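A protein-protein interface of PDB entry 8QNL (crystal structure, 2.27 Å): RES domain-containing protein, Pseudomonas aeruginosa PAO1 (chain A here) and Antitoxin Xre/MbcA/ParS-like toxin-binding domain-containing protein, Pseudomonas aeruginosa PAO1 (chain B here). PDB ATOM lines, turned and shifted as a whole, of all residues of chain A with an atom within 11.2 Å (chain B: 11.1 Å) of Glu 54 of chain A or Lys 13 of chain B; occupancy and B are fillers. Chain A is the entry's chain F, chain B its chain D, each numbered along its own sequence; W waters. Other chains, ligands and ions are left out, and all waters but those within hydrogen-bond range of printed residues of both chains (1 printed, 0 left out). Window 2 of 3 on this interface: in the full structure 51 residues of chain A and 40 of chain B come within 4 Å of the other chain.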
ATOM      1  N   GLN A  43      20.339 -40.809  14.898  1.00  0.00           N
ATOM      2  CA  GLN A  43      20.705 -39.406  14.742  1.00  0.00           C
ATOM      3  C   GLN A  43      21.262 -39.128  13.354  1.00  0.00           C
ATOM      4  O   GLN A  43      21.054 -38.036  12.813  1.00  0.00           O
ATOM      5  CB  GLN A  43      21.719 -38.998  15.814  1.00  0.00           C
ATOM      6  CG  GLN A  43      21.194 -39.120  17.231  1.00  0.00           C
ATOM      7  CD  GLN A  43      21.152 -37.790  17.956  1.00  0.00           C
ATOM      8  OE1 GLN A  43      20.539 -36.830  17.491  1.00  0.00           O
ATOM      9  NE2 GLN A  43      21.810 -37.728  19.104  1.00  0.00           N
ATOM     10  N   THR A  46      18.178 -38.451  10.948  1.00  0.00           N
ATOM     11  CA  THR A  46      17.599 -37.113  10.905  1.00  0.00           C
ATOM     12  C   THR A  46      18.570 -36.078  10.352  1.00  0.00           C
ATOM     13  O   THR A  46      18.125 -35.047   9.835  1.00  0.00           O
ATOM     14  CB  THR A  46      17.123 -36.694  12.295  1.00  0.00           C
ATOM     15  OG1 THR A  46      18.160 -36.944  13.249  1.00  0.00           O
ATOM     16  CG2 THR A  46      15.881 -37.486  12.679  1.00  0.00           C
ATOM     17  N   LEU A  47      19.879 -36.331  10.435  1.00  0.00           N
ATOM     18  CA  LEU A  47      20.842 -35.410   9.840  1.00  0.00           C
ATOM     19  C   LEU A  47      20.716 -35.374   8.319  1.00  0.00           C
ATOM     20  O   LEU A  47      21.050 -34.358   7.698  1.00  0.00           O
ATOM     21  CB  LEU A  47      22.263 -35.790  10.267  1.00  0.00           C
ATOM     22  CG  LEU A  47      23.368 -34.807   9.870  1.00  0.00           C
ATOM     23  CD1 LEU A  47      23.009 -33.381  10.278  1.00  0.00           C
ATOM     24  CD2 LEU A  47      24.707 -35.212  10.474  1.00  0.00           C
ATOM     25  N   GLN A  48      20.226 -36.459   7.704  1.00  0.00           N
ATOM     26  CA  GLN A  48      19.979 -36.468   6.264  1.00  0.00           C
ATOM     27  C   GLN A  48      18.801 -35.585   5.864  1.00  0.00           C
ATOM     28  O   GLN A  48      18.725 -35.167   4.701  1.00  0.00           O
ATOM     29  CB  GLN A  48      19.722 -37.901   5.771  1.00  0.00           C
ATOM     30  CG  GLN A  48      20.744 -38.934   6.228  1.00  0.00           C
ATOM     31  CD  GLN A  48      22.156 -38.570   5.825  1.00  0.00           C
ATOM     32  OE1 GLN A  48      23.078 -38.627   6.639  1.00  0.00           O
ATOM     33  NE2 GLN A  48      22.335 -38.193   4.565  1.00  0.00           N
ATOM     34  N   LEU A  49      17.886 -35.296   6.795  1.00  0.00           N
ATOM     35  CA  LEU A  49      16.687 -34.518   6.502  1.00  0.00           C
ATOM     36  C   LEU A  49      16.909 -33.013   6.541  1.00  0.00           C
ATOM     37  O   LEU A  49      16.136 -32.276   5.921  1.00  0.00           O
ATOM     38  CB  LEU A  49      15.577 -34.871   7.498  1.00  0.00           C
ATOM     39  CG  LEU A  49      15.107 -36.322   7.482  1.00  0.00           C
ATOM     40  CD1 LEU A  49      13.915 -36.503   8.408  1.00  0.00           C
ATOM     41  CD2 LEU A  49      14.777 -36.766   6.061  1.00  0.00           C
ATOM     42  N   VAL A  50      17.924 -32.539   7.266  1.00  0.00           N
ATOM     43  CA  VAL A  50      18.150 -31.108   7.443  1.00  0.00           C
ATOM     44  C   VAL A  50      19.533 -30.738   6.922  1.00  0.00           C
ATOM     45  O   VAL A  50      20.245 -31.580   6.365  1.00  0.00           O
ATOM     46  CB  VAL A  50      17.990 -30.696   8.920  1.00  0.00           C
ATOM     47  CG1 VAL A  50      16.567 -30.950   9.391  1.00  0.00           C
ATOM     48  CG2 VAL A  50      18.993 -31.444   9.788  1.00  0.00           C
ATOM     49  N   ASP A  51      19.927 -29.480   7.112  1.00  0.00           N
ATOM     50  CA  ASP A  51      21.165 -28.966   6.542  1.00  0.00           C
ATOM     51  C   ASP A  51      22.281 -28.754   7.552  1.00  0.00           C
ATOM     52  O   ASP A  51      23.451 -28.853   7.180  1.00  0.00           O
ATOM     53  CB  ASP A  51      20.900 -27.642   5.815  1.00  0.00           C
ATOM     54  CG  ASP A  51      20.033 -27.821   4.581  1.00  0.00           C
ATOM     55  OD1 ASP A  51      20.273 -28.783   3.822  1.00  0.00           O
ATOM     56  OD2 ASP A  51      19.107 -27.006   4.375  1.00  0.00           O
ATOM     57  N   THR A  52      21.962 -28.465   8.810  1.00  0.00           N
ATOM     58  CA  THR A  52      22.973 -28.195   9.822  1.00  0.00           C
ATOM     59  C   THR A  52      22.742 -29.086  11.034  1.00  0.00           C
ATOM     60  O   THR A  52      21.646 -29.611  11.246  1.00  0.00           O
ATOM     61  CB  THR A  52      22.964 -26.724  10.259  1.00  0.00           C
ATOM     62  OG1 THR A  52      21.736 -26.433  10.937  1.00  0.00           O
ATOM     63  CG2 THR A  52      23.112 -25.797   9.056  1.00  0.00           C
ATOM     64  N   LEU A  53      23.798 -29.248  11.837  1.00  0.00           N
ATOM     65  CA  LEU A  53      23.645 -29.937  13.113  1.00  0.00           C
ATOM     66  C   LEU A  53      22.736 -29.156  14.050  1.00  0.00           C
ATOM     67  O   LEU A  53      22.027 -29.753  14.870  1.00  0.00           O
ATOM     68  CB  LEU A  53      25.009 -30.162  13.769  1.00  0.00           C
ATOM     69  CG  LEU A  53      25.902 -31.268  13.199  1.00  0.00           C
ATOM     70  CD1 LEU A  53      27.158 -31.436  14.051  1.00  0.00           C
ATOM     71  CD2 LEU A  53      25.142 -32.579  13.109  1.00  0.00           C
ATOM     72  N   GLU A  54      22.744 -27.824  13.946  1.00  0.00           N
ATOM     73  CA  GLU A  54      21.855 -27.015  14.773  1.00  0.00           C
ATOM     74  C   GLU A  54      20.395 -27.278  14.423  1.00  0.00           C
ATOM     75  O   GLU A  54      19.543 -27.348  15.316  1.00  0.00           O
ATOM     76  CB  GLU A  54      22.194 -25.531  14.615  1.00  0.00           C
ATOM     77  CG  GLU A  54      21.672 -24.643  15.736  1.00  0.00           C
ATOM     78  CD  GLU A  54      22.419 -24.842  17.049  1.00  0.00           C
ATOM     79  OE1 GLU A  54      22.030 -25.734  17.835  1.00  0.00           O
ATOM     80  OE2 GLU A  54      23.400 -24.103  17.292  1.00  0.00           O
ATOM     81  N   GLU A  55      20.085 -27.426  13.132  1.00  0.00           N
ATOM     82  CA  GLU A  55      18.728 -27.795  12.749  1.00  0.00           C
ATOM     83  C   GLU A  55      18.401 -29.223  13.163  1.00  0.00           C
ATOM     84  O   GLU A  55      17.266 -29.507  13.564  1.00  0.00           O
ATOM     85  CB  GLU A  55      18.536 -27.620  11.244  1.00  0.00           C
ATOM     86  CG  GLU A  55      18.525 -26.170  10.778  1.00  0.00           C
ATOM     87  CD  GLU A  55      18.287 -26.044   9.286  1.00  0.00           C
ATOM     88  OE1 GLU A  55      18.515 -27.034   8.557  1.00  0.00           O
ATOM     89  OE2 GLU A  55      17.865 -24.956   8.843  1.00  0.00           O
ATOM     90  N   GLN A  56      19.379 -30.129  13.085  1.00  0.00           N
ATOM     91  CA  GLN A  56      19.137 -31.516  13.468  1.00  0.00           C
ATOM     92  C   GLN A  56      18.850 -31.635  14.961  1.00  0.00           C
ATOM     93  O   GLN A  56      18.010 -32.442  15.373  1.00  0.00           O
ATOM     94  CB  GLN A  56      20.332 -32.385  13.067  1.00  0.00           C
ATOM     95  CG  GLN A  56      20.073 -33.892  13.084  1.00  0.00           C
ATOM     96  CD  GLN A  56      20.443 -34.542  14.404  1.00  0.00           C
ATOM     97  OE1 GLN A  56      20.752 -33.858  15.375  1.00  0.00           O
ATOM     98  NE2 GLN A  56      20.420 -35.872  14.442  1.00  0.00           N
ATOM     99  N   ALA A  57      19.532 -30.834  15.786  1.00  0.00           N
ATOM    100  CA  ALA A  57      19.287 -30.879  17.225  1.00  0.00           C
ATOM    101  C   ALA A  57      17.897 -30.357  17.564  1.00  0.00           C
ATOM    102  O   ALA A  57      17.244 -30.861  18.485  1.00  0.00           O
ATOM    103  CB  ALA A  57      20.358 -30.079  17.969  1.00  0.00           C
ATOM    104  N   LEU A  58      17.429 -29.342  16.834  1.00  0.00           N
ATOM    105  CA  LEU A  58      16.071 -28.853  17.039  1.00  0.00           C
ATOM    106  C   LEU A  58      15.042 -29.867  16.544  1.00  0.00           C
ATOM    107  O   LEU A  58      14.011 -30.082  17.194  1.00  0.00           O
ATOM    108  CB  LEU A  58      15.891 -27.504  16.341  1.00  0.00           C
ATOM    109  CG  LEU A  58      14.498 -26.872  16.402  1.00  0.00           C
ATOM    110  CD1 LEU A  58      14.088 -26.634  17.850  1.00  0.00           C
ATOM    111  CD2 LEU A  58      14.447 -25.573  15.600  1.00  0.00           C
ATOM    112  N   LEU A  59      15.307 -30.506  15.401  1.00  0.00           N
ATOM    113  CA  LEU A  59      14.405 -31.549  14.917  1.00  0.00           C
ATOM    114  C   LEU A  59      14.290 -32.691  15.921  1.00  0.00           C
ATOM    115  O   LEU A  59      13.184 -33.163  16.209  1.00  0.00           O
ATOM    116  CB  LEU A  59      14.876 -32.070  13.560  1.00  0.00           C
ATOM    117  CG  LEU A  59      14.042 -33.198  12.945  1.00  0.00           C
ATOM    118  CD1 LEU A  59      12.604 -32.747  12.714  1.00  0.00           C
ATOM    119  CD2 LEU A  59      14.671 -33.685  11.648  1.00  0.00           C
ATOM    120  N   GLU A  60      15.420 -33.133  16.481  1.00  0.00           N
ATOM    121  CA  GLU A  60      15.384 -34.191  17.487  1.00  0.00           C
ATOM    122  C   GLU A  60      14.609 -33.762  18.729  1.00  0.00           C
ATOM    123  O   GLU A  60      13.983 -34.603  19.386  1.00  0.00           O
ATOM    124  CB  GLU A  60      16.807 -34.618  17.849  1.00  0.00           C
ATOM    125  CG  GLU A  60      17.476 -35.522  16.801  1.00  0.00           C
ATOM    126  CD  GLU A  60      16.909 -36.936  16.799  1.00  0.00           C
ATOM    127  OE1 GLU A  60      16.428 -37.385  17.858  1.00  0.00           O
ATOM    128  OE2 GLU A  60      16.946 -37.597  15.738  1.00  0.00           O
ATOM    129  N   GLU A  61      14.618 -32.466  19.061  1.00  0.00           N
ATOM    130  CA  GLU A  61      13.779 -31.981  20.157  1.00  0.00           C
ATOM    131  C   GLU A  61      12.300 -32.021  19.785  1.00  0.00           C
ATOM    132  O   GLU A  61      11.451 -32.335  20.629  1.00  0.00           O
ATOM    133  CB  GLU A  61      14.191 -30.561  20.559  1.00  0.00           C
ATOM    134  CG  GLU A  61      15.478 -30.488  21.367  1.00  0.00           C
ATOM    135  CD  GLU A  61      16.040 -29.076  21.460  1.00  0.00           C
ATOM    136  OE1 GLU A  61      17.070 -28.802  20.804  1.00  0.00           O
ATOM    137  OE2 GLU A  61      15.452 -28.239  22.181  1.00  0.00           O
ATOM    138  N   LEU A  62      11.963 -31.697  18.533  1.00  0.00           N
ATOM    139  CA  LEU A  62      10.568 -31.787  18.113  1.00  0.00           C
ATOM    140  C   LEU A  62      10.089 -33.232  18.127  1.00  0.00           C
ATOM    141  O   LEU A  62       8.971 -33.515  18.574  1.00  0.00           O
ATOM    142  CB  LEU A  62      10.389 -31.179  16.723  1.00  0.00           C
ATOM    143  CG  LEU A  62      10.861 -29.739  16.533  1.00  0.00           C
ATOM    144  CD1 LEU A  62      10.577 -29.261  15.115  1.00  0.00           C
ATOM    145  CD2 LEU A  62      10.213 -28.822  17.560  1.00  0.00           C
ATOM    146  N   LEU B   4      37.864 -15.295  22.282  1.00  0.00           N
ATOM    147  CA  LEU B   4      37.914 -15.693  20.879  1.00  0.00           C
ATOM    148  C   LEU B   4      36.800 -16.678  20.547  1.00  0.00           C
ATOM    149  O   LEU B   4      36.142 -16.552  19.507  1.00  0.00           O
ATOM    150  CB  LEU B   4      39.279 -16.299  20.558  1.00  0.00           C
ATOM    151  CG  LEU B   4      39.462 -16.809  19.130  1.00  0.00           C
ATOM    152  CD1 LEU B   4      39.351 -15.658  18.141  1.00  0.00           C
ATOM    153  CD2 LEU B   4      40.798 -17.533  18.985  1.00  0.00           C
ATOM    154  N   ASN B   5      36.565 -17.650  21.404  1.00  0.00           N
ATOM    155  CA  ASN B   5      35.458 -18.599  21.154  1.00  0.00           C
ATOM    156  C   ASN B   5      34.108 -17.874  21.229  1.00  0.00           C
ATOM    157  O   ASN B   5      33.248 -18.174  20.411  1.00  0.00           O
ATOM    158  CB  ASN B   5      35.548 -19.825  22.061  1.00  0.00           C
ATOM    159  CG  ASN B   5      35.136 -21.103  21.357  1.00  0.00           C
ATOM    160  OD1 ASN B   5      34.617 -21.071  20.245  1.00  0.00           O
ATOM    161  ND2 ASN B   5      35.361 -22.234  22.001  1.00  0.00           N
ATOM    162  N   TRP B   6      33.945 -16.952  22.173  1.00  0.00           N
ATOM    163  CA  TRP B   6      32.649 -16.300  22.325  1.00  0.00           C
ATOM    164  C   TRP B   6      32.268 -15.529  21.067  1.00  0.00           C
ATOM    165  O   TRP B   6      31.166 -15.697  20.534  1.00  0.00           O
ATOM    166  CB  TRP B   6      32.667 -15.378  23.545  1.00  0.00           C
ATOM    167  CG  TRP B   6      31.351 -14.728  23.819  1.00  0.00           C
ATOM    168  CD1 TRP B   6      30.322 -15.236  24.562  1.00  0.00           C
ATOM    169  CD2 TRP B   6      30.915 -13.449  23.352  1.00  0.00           C
ATOM    170  NE1 TRP B   6      29.274 -14.348  24.585  1.00  0.00           N
ATOM    171  CE2 TRP B   6      29.612 -13.242  23.849  1.00  0.00           C
ATOM    172  CE3 TRP B   6      31.499 -12.455  22.559  1.00  0.00           C
ATOM    173  CZ2 TRP B   6      28.886 -12.084  23.582  1.00  0.00           C
ATOM    174  CZ3 TRP B   6      30.778 -11.309  22.295  1.00  0.00           C
ATOM    175  CH2 TRP B   6      29.485 -11.133  22.804  1.00  0.00           C
ATOM    176  N   ILE B   7      33.176 -14.684  20.571  1.00  0.00           N
ATOM    177  CA  ILE B   7      32.848 -13.865  19.411  1.00  0.00           C
ATOM    178  C   ILE B   7      32.778 -14.712  18.145  1.00  0.00           C
ATOM    179  O   ILE B   7      31.990 -14.416  17.240  1.00  0.00           O
ATOM    180  CB  ILE B   7      33.856 -12.711  19.266  1.00  0.00           C
ATOM    181  CG1 ILE B   7      33.367 -11.708  18.220  1.00  0.00           C
ATOM    182  CG2 ILE B   7      35.235 -13.235  18.903  1.00  0.00           C
ATOM    183  CD1 ILE B   7      32.100 -10.990  18.619  1.00  0.00           C
ATOM    184  N   SER B   8      33.587 -15.771  18.053  1.00  0.00           N
ATOM    185  CA  SER B   8      33.558 -16.605  16.856  1.00  0.00           C
ATOM    186  C   SER B   8      32.231 -17.334  16.733  1.00  0.00           C
ATOM    187  O   SER B   8      31.653 -17.406  15.642  1.00  0.00           O
ATOM    188  CB  SER B   8      34.709 -17.605  16.879  1.00  0.00           C
ATOM    189  OG  SER B   8      35.943 -16.947  16.675  1.00  0.00           O
ATOM    190  N   SER B   9      31.734 -17.879  17.842  1.00  0.00           N
ATOM    191  CA  SER B   9      30.446 -18.558  17.816  1.00  0.00           C
ATOM    192  C   SER B   9      29.301 -17.578  17.590  1.00  0.00           C
ATOM    193  O   SER B   9      28.315 -17.924  16.931  1.00  0.00           O
ATOM    194  CB  SER B   9      30.239 -19.336  19.117  1.00  0.00           C
ATOM    195  OG  SER B   9      31.235 -20.333  19.279  1.00  0.00           O
ATOM    196  N   ALA B  10      29.416 -16.354  18.113  1.00  0.00           N
ATOM    197  CA  ALA B  10      28.332 -15.389  17.955  1.00  0.00           C
ATOM    198  C   ALA B  10      28.178 -14.942  16.506  1.00  0.00           C
ATOM    199  O   ALA B  10      27.062 -14.634  16.073  1.00  0.00           O
ATOM    200  CB  ALA B  10      28.561 -14.181  18.865  1.00  0.00           C
ATOM    201  N   LEU B  11      29.273 -14.907  15.745  1.00  0.00           N
ATOM    202  CA  LEU B  11      29.220 -14.478  14.353  1.00  0.00           C
ATOM    203  C   LEU B  11      28.615 -15.525  13.431  1.00  0.00           C
ATOM    204  O   LEU B  11      28.193 -15.183  12.323  1.00  0.00           O
ATOM    205  CB  LEU B  11      30.621 -14.124  13.855  1.00  0.00           C
ATOM    206  CG  LEU B  11      31.286 -12.909  14.500  1.00  0.00           C
ATOM    207  CD1 LEU B  11      32.717 -12.776  14.016  1.00  0.00           C
ATOM    208  CD2 LEU B  11      30.498 -11.638  14.217  1.00  0.00           C
ATOM    209  N   ILE B  12      28.567 -16.788  13.852  1.00  0.00           N
ATOM    210  CA  ILE B  12      28.090 -17.869  13.000  1.00  0.00           C
ATOM    211  C   ILE B  12      26.903 -18.610  13.593  1.00  0.00           C
ATOM    212  O   ILE B  12      26.428 -19.576  12.987  1.00  0.00           O
ATOM    213  CB  ILE B  12      29.221 -18.866  12.678  1.00  0.00           C
ATOM    214  CG1 ILE B  12      29.650 -19.600  13.944  1.00  0.00           C
ATOM    215  CG2 ILE B  12      30.412 -18.150  12.064  1.00  0.00           C
ATOM    216  CD1 ILE B  12      30.666 -20.666  13.682  1.00  0.00           C
ATOM    217  N   LYS B  13      26.403 -18.192  14.755  1.00  0.00           N
ATOM    218  CA  LYS B  13      25.351 -18.948  15.419  1.00  0.00           C
ATOM    219  C   LYS B  13      24.062 -18.893  14.612  1.00  0.00           C
ATOM    220  O   LYS B  13      23.638 -17.824  14.160  1.00  0.00           O
ATOM    221  CB  LYS B  13      25.113 -18.417  16.832  1.00  0.00           C
ATOM    222  CG  LYS B  13      24.504 -19.450  17.779  1.00  0.00           C
ATOM    223  CD  LYS B  13      25.346 -20.728  17.826  1.00  0.00           C
ATOM    224  CE  LYS B  13      26.760 -20.462  18.341  1.00  0.00           C
ATOM    225  NZ  LYS B  13      27.705 -21.576  18.032  1.00  0.00           N
ATOM    226  N   GLU B  14      23.444 -20.053  14.429  1.00  0.00           N
ATOM    227  CA  GLU B  14      22.187 -20.176  13.710  1.00  0.00           C
ATOM    228  C   GLU B  14      21.076 -20.502  14.699  1.00  0.00           C
ATOM    229  O   GLU B  14      21.227 -21.402  15.533  1.00  0.00           O
ATOM    230  CB  GLU B  14      22.293 -21.257  12.633  1.00  0.00           C
ATOM    231  CG  GLU B  14      23.418 -22.253  12.883  1.00  0.00           C
ATOM    232  CD  GLU B  14      23.368 -23.434  11.936  1.00  0.00           C
ATOM    233  OE1 GLU B  14      22.288 -23.673  11.353  1.00  0.00           O
ATOM    234  OE2 GLU B  14      24.403 -24.120  11.775  1.00  0.00           O
ATOM    235  N   ARG B  15      19.971 -19.754  14.617  1.00  0.00           N
ATOM    236  CA  ARG B  15      18.787 -19.970  15.450  1.00  0.00           C
ATOM    237  C   ARG B  15      17.634 -20.377  14.535  1.00  0.00           C
ATOM    238  O   ARG B  15      16.802 -19.538  14.152  1.00  0.00           O
ATOM    239  CB  ARG B  15      18.451 -18.721  16.267  1.00  0.00           C
ATOM    240  CG  ARG B  15      19.681 -18.040  16.875  1.00  0.00           C
ATOM    241  CD  ARG B  15      19.333 -16.941  17.871  1.00  0.00           C
ATOM    242  NE  ARG B  15      19.093 -17.532  19.179  1.00  0.00           N
ATOM    243  CZ  ARG B  15      20.043 -17.770  20.078  1.00  0.00           C
ATOM    244  NH1 ARG B  15      21.306 -17.443  19.828  1.00  0.00           N
ATOM    245  NH2 ARG B  15      19.727 -18.333  21.234  1.00  0.00           N
ATOM    246  N   PRO B  16      17.547 -21.656  14.173  1.00  0.00           N
ATOM    247  CA  PRO B  16      16.559 -22.083  13.172  1.00  0.00           C
ATOM    248  C   PRO B  16      15.137 -22.061  13.716  1.00  0.00           C
ATOM    249  O   PRO B  16      14.892 -22.188  14.918  1.00  0.00           O
ATOM    250  CB  PRO B  16      16.997 -23.512  12.832  1.00  0.00           C
ATOM    251  CG  PRO B  16      17.692 -23.984  14.065  1.00  0.00           C
ATOM    252  CD  PRO B  16      18.374 -22.776  14.653  1.00  0.00           C
ATOM    253  N   SER B  17      14.192 -21.908  12.791  1.00  0.00           N
ATOM    254  CA  SER B  17      12.774 -21.900  13.127  1.00  0.00           C
ATOM    255  C   SER B  17      12.239 -23.321  13.246  1.00  0.00           C
ATOM    256  O   SER B  17      12.525 -24.178  12.407  1.00  0.00           O
ATOM    257  CB  SER B  17      11.986 -21.134  12.065  1.00  0.00           C
ATOM    258  OG  SER B  17      10.603 -21.449  12.123  1.00  0.00           O
ATOM    259  N   ALA B  18      11.449 -23.568  14.295  1.00  0.00           N
ATOM    260  CA  ALA B  18      10.881 -24.898  14.497  1.00  0.00           C
ATOM    261  C   ALA B  18       9.942 -25.285  13.357  1.00  0.00           C
ATOM    262  O   ALA B  18      10.032 -26.398  12.824  1.00  0.00           O
ATOM    263  CB  ALA B  18      10.156 -24.962  15.839  1.00  0.00           C
ATOM    264  N   ALA B  20       9.874 -24.113  10.297  1.00  0.00           N
ATOM    265  CA  ALA B  20      10.620 -24.255   9.048  1.00  0.00           C
ATOM    266  C   ALA B  20      11.446 -25.535   9.036  1.00  0.00           C
ATOM    267  O   ALA B  20      11.590 -26.177   7.989  1.00  0.00           O
ATOM    268  CB  ALA B  20      11.522 -23.039   8.834  1.00  0.00           C
ATOM    269  N   VAL B  21      12.007 -25.910  10.186  1.00  0.00           N
ATOM    270  CA  VAL B  21      12.794 -27.137  10.267  1.00  0.00           C
ATOM    271  C   VAL B  21      11.906 -28.359  10.053  1.00  0.00           C
ATOM    272  O   VAL B  21      12.273 -29.288   9.323  1.00  0.00           O
ATOM    273  CB  VAL B  21      13.539 -27.200  11.613  1.00  0.00           C
ATOM    274  CG1 VAL B  21      13.921 -28.630  11.946  1.00  0.00           C
ATOM    275  CG2 VAL B  21      14.780 -26.311  11.573  1.00  0.00           C
ATOM    276  N   LEU B  22      10.724 -28.378  10.677  1.00  0.00           N
ATOM    277  CA  LEU B  22       9.816 -29.507  10.492  1.00  0.00           C
ATOM    278  C   LEU B  22       9.338 -29.599   9.049  1.00  0.00           C
ATOM    279  O   LEU B  22       9.262 -30.696   8.485  1.00  0.00           O
ATOM    280  CB  LEU B  22       8.623 -29.398  11.444  1.00  0.00           C
ATOM    281  CG  LEU B  22       7.617 -30.556  11.399  1.00  0.00           C
ATOM    282  CD1 LEU B  22       8.319 -31.889  11.593  1.00  0.00           C
ATOM    283  CD2 LEU B  22       6.516 -30.379  12.440  1.00  0.00           C
ATOM    284  N   LYS B  24      10.910 -28.610   6.346  1.00  0.00           N
ATOM    285  CA  LYS B  24      12.023 -29.151   5.572  1.00  0.00           C
ATOM    286  C   LYS B  24      12.236 -30.634   5.849  1.00  0.00           C
ATOM    287  O   LYS B  24      12.543 -31.395   4.925  1.00  0.00           O
ATOM    288  CB  LYS B  24      13.298 -28.360   5.881  1.00  0.00           C
ATOM    289  CG  LYS B  24      14.550 -28.872   5.185  1.00  0.00           C
ATOM    290  CD  LYS B  24      15.812 -28.211   5.736  1.00  0.00           C
ATOM    291  CE  LYS B  24      15.773 -26.704   5.565  1.00  0.00           C
ATOM    292  NZ  LYS B  24      16.995 -26.051   6.120  1.00  0.00           N
ATOM    293  N   ALA B  25      12.050 -31.068   7.099  1.00  0.00           N
ATOM    294  CA  ALA B  25      12.301 -32.463   7.449  1.00  0.00           C
ATOM    295  C   ALA B  25      11.266 -33.398   6.835  1.00  0.00           C
ATOM    296  O   ALA B  25      11.614 -34.490   6.375  1.00  0.00           O
ATOM    297  CB  ALA B  25      12.328 -32.628   8.968  1.00  0.00           C
HETATM  298  O   HOH W   1      25.225 -26.664  12.734  1.00  0.00           O
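NZ of Lys 24 of chain B is in salt-bridge range of OD2 of Asp 51 of chain A (2.9 Å). NZ of Lys 24 of chain B lies within salt-bridge range of OE1 of Glu 55 of chain A (3.0 Å). OE1 of Glu 14 of chain B lies within hydrogen-bond range of OG1 of Thr 52 of chain A (2.8 Å).
N of Ala 20 of chain B sits at hydrogen-bond distance from OG of Ser 17 of chain B (3.3 Å). The side-chain hydroxyl (OG1) of Thr 52 of chain A lies close to the backbone NH (N) of Glu 54 of chain A (3.5 Å). The side-chain hydroxyl of Thr 52 of chain A is in hydrogen-bond range of the backbone NH of Glu 55 of chain A, 2.9 Å away. The side-chain carboxylate (OE1) of Glu 55 of chain A lies within hydrogen-bond range of the backbone NH (N) of Asp 51 of chain A, 3.2 Å away.
CG of Lys 24 of chain B touches O of Leu 49 of chain A (3.8 Å). Leu 49 of chain A touches Ala 25 of chain B. Lys 13 of chain B touches Glu 54 of chain A (CD to OE2, 3.9 Å). CG of Glu 54 of chain A touches O of Glu 14 of chain B, 3.3 Å away. Pro 16 of chain B touches Glu 54 of chain A (CD to CG, 3.9 Å). Glu 55 of chain A touches Pro 16 of chain B (CG to CB, 3.7 Å). Pro 16 of chain B touches Leu 58 of chain A. Leu 59 of chain A touches Val 21 of chain B. Leu 59 of chain A touches Ala 25 of chain B. Leu 62 of chain A touches Ala 18 of chain B (CD1 to O, 3.7 Å).
Of the printed residues of chain B, Asp 51 of chain A touches Lys 24. Of chain B, only Glu 14 (2.8 Å) comes within 4 Å of Thr 52 of chain A. Of chain B, only Lys 13, Glu 14 and Pro 16 come within 4 Å of Glu 54 of chain A. Of chain B, only Pro 16, Val 21 and Lys 24 come within 4 Å of Glu 55 of chain A. No residue of chain B comes within 4 Å of Ala 57 of chain A. Of chain B, only Pro 16 (3.5 Å), Ser 17 (3.9 Å) and Ala 18 (3.8 Å) come within 4 Å of Leu 58 of chain A. Printed residues of chain B within 4 Å of Leu 62 of chain A: Ala 18. No residue of chain A comes within 4 Å of Ser 9 of chain B. No residue of chain A comes within 4 Å of Ala 10 of chain B. Of the printed residues of chain A, Lys 13 of chain B touches Glu 54. Glu 14 of chain B touches two residues of chain A. No residue of chain A comes within 4 Å of Arg 15 of chain B. Of the printed residues of chain A, Ser 17 of chain B touches Leu 58 (3.9 Å). Of the printed residues of chain A, Ala 25 of chain B touches Leu 49 (3.7 Å) and Leu 59 (3.7 Å). The nearest residue of chain B that does not touch Glu 54 of chain A is Arg 15 of chain B (5.3 Å). The nearest printed residue of chain B that does not touch Leu 59 of chain A is Leu 22 of chain B (4.5 Å).
Of the 20 printed residues of chain B, 8 touch a printed residue of chain A. Hydrophobic or aromatic side chains of chain B that line the printed part of chain A: Pro 16, Val 21 and Ala 25. Hydrophobic or aromatic side chains of chain A that line the printed part of chain B: Leu 49, Leu 58, Leu 59 and Leu 62. Among the printed residues, Asp or Glu carboxylates within 4 Å of a Lys or Arg side-chain nitrogen of the other chain: Asp 51 of chain A with Lys 24 of chain B and Glu 55 of chain A with Lys 24 of chain B.
Water W1 lies within hydrogen-bond range of the side-chain carboxylate of Glu 14 of chain B, the backbone NH of Glu 54 of chain A and the backbone NH of Leu 53 of chain A.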
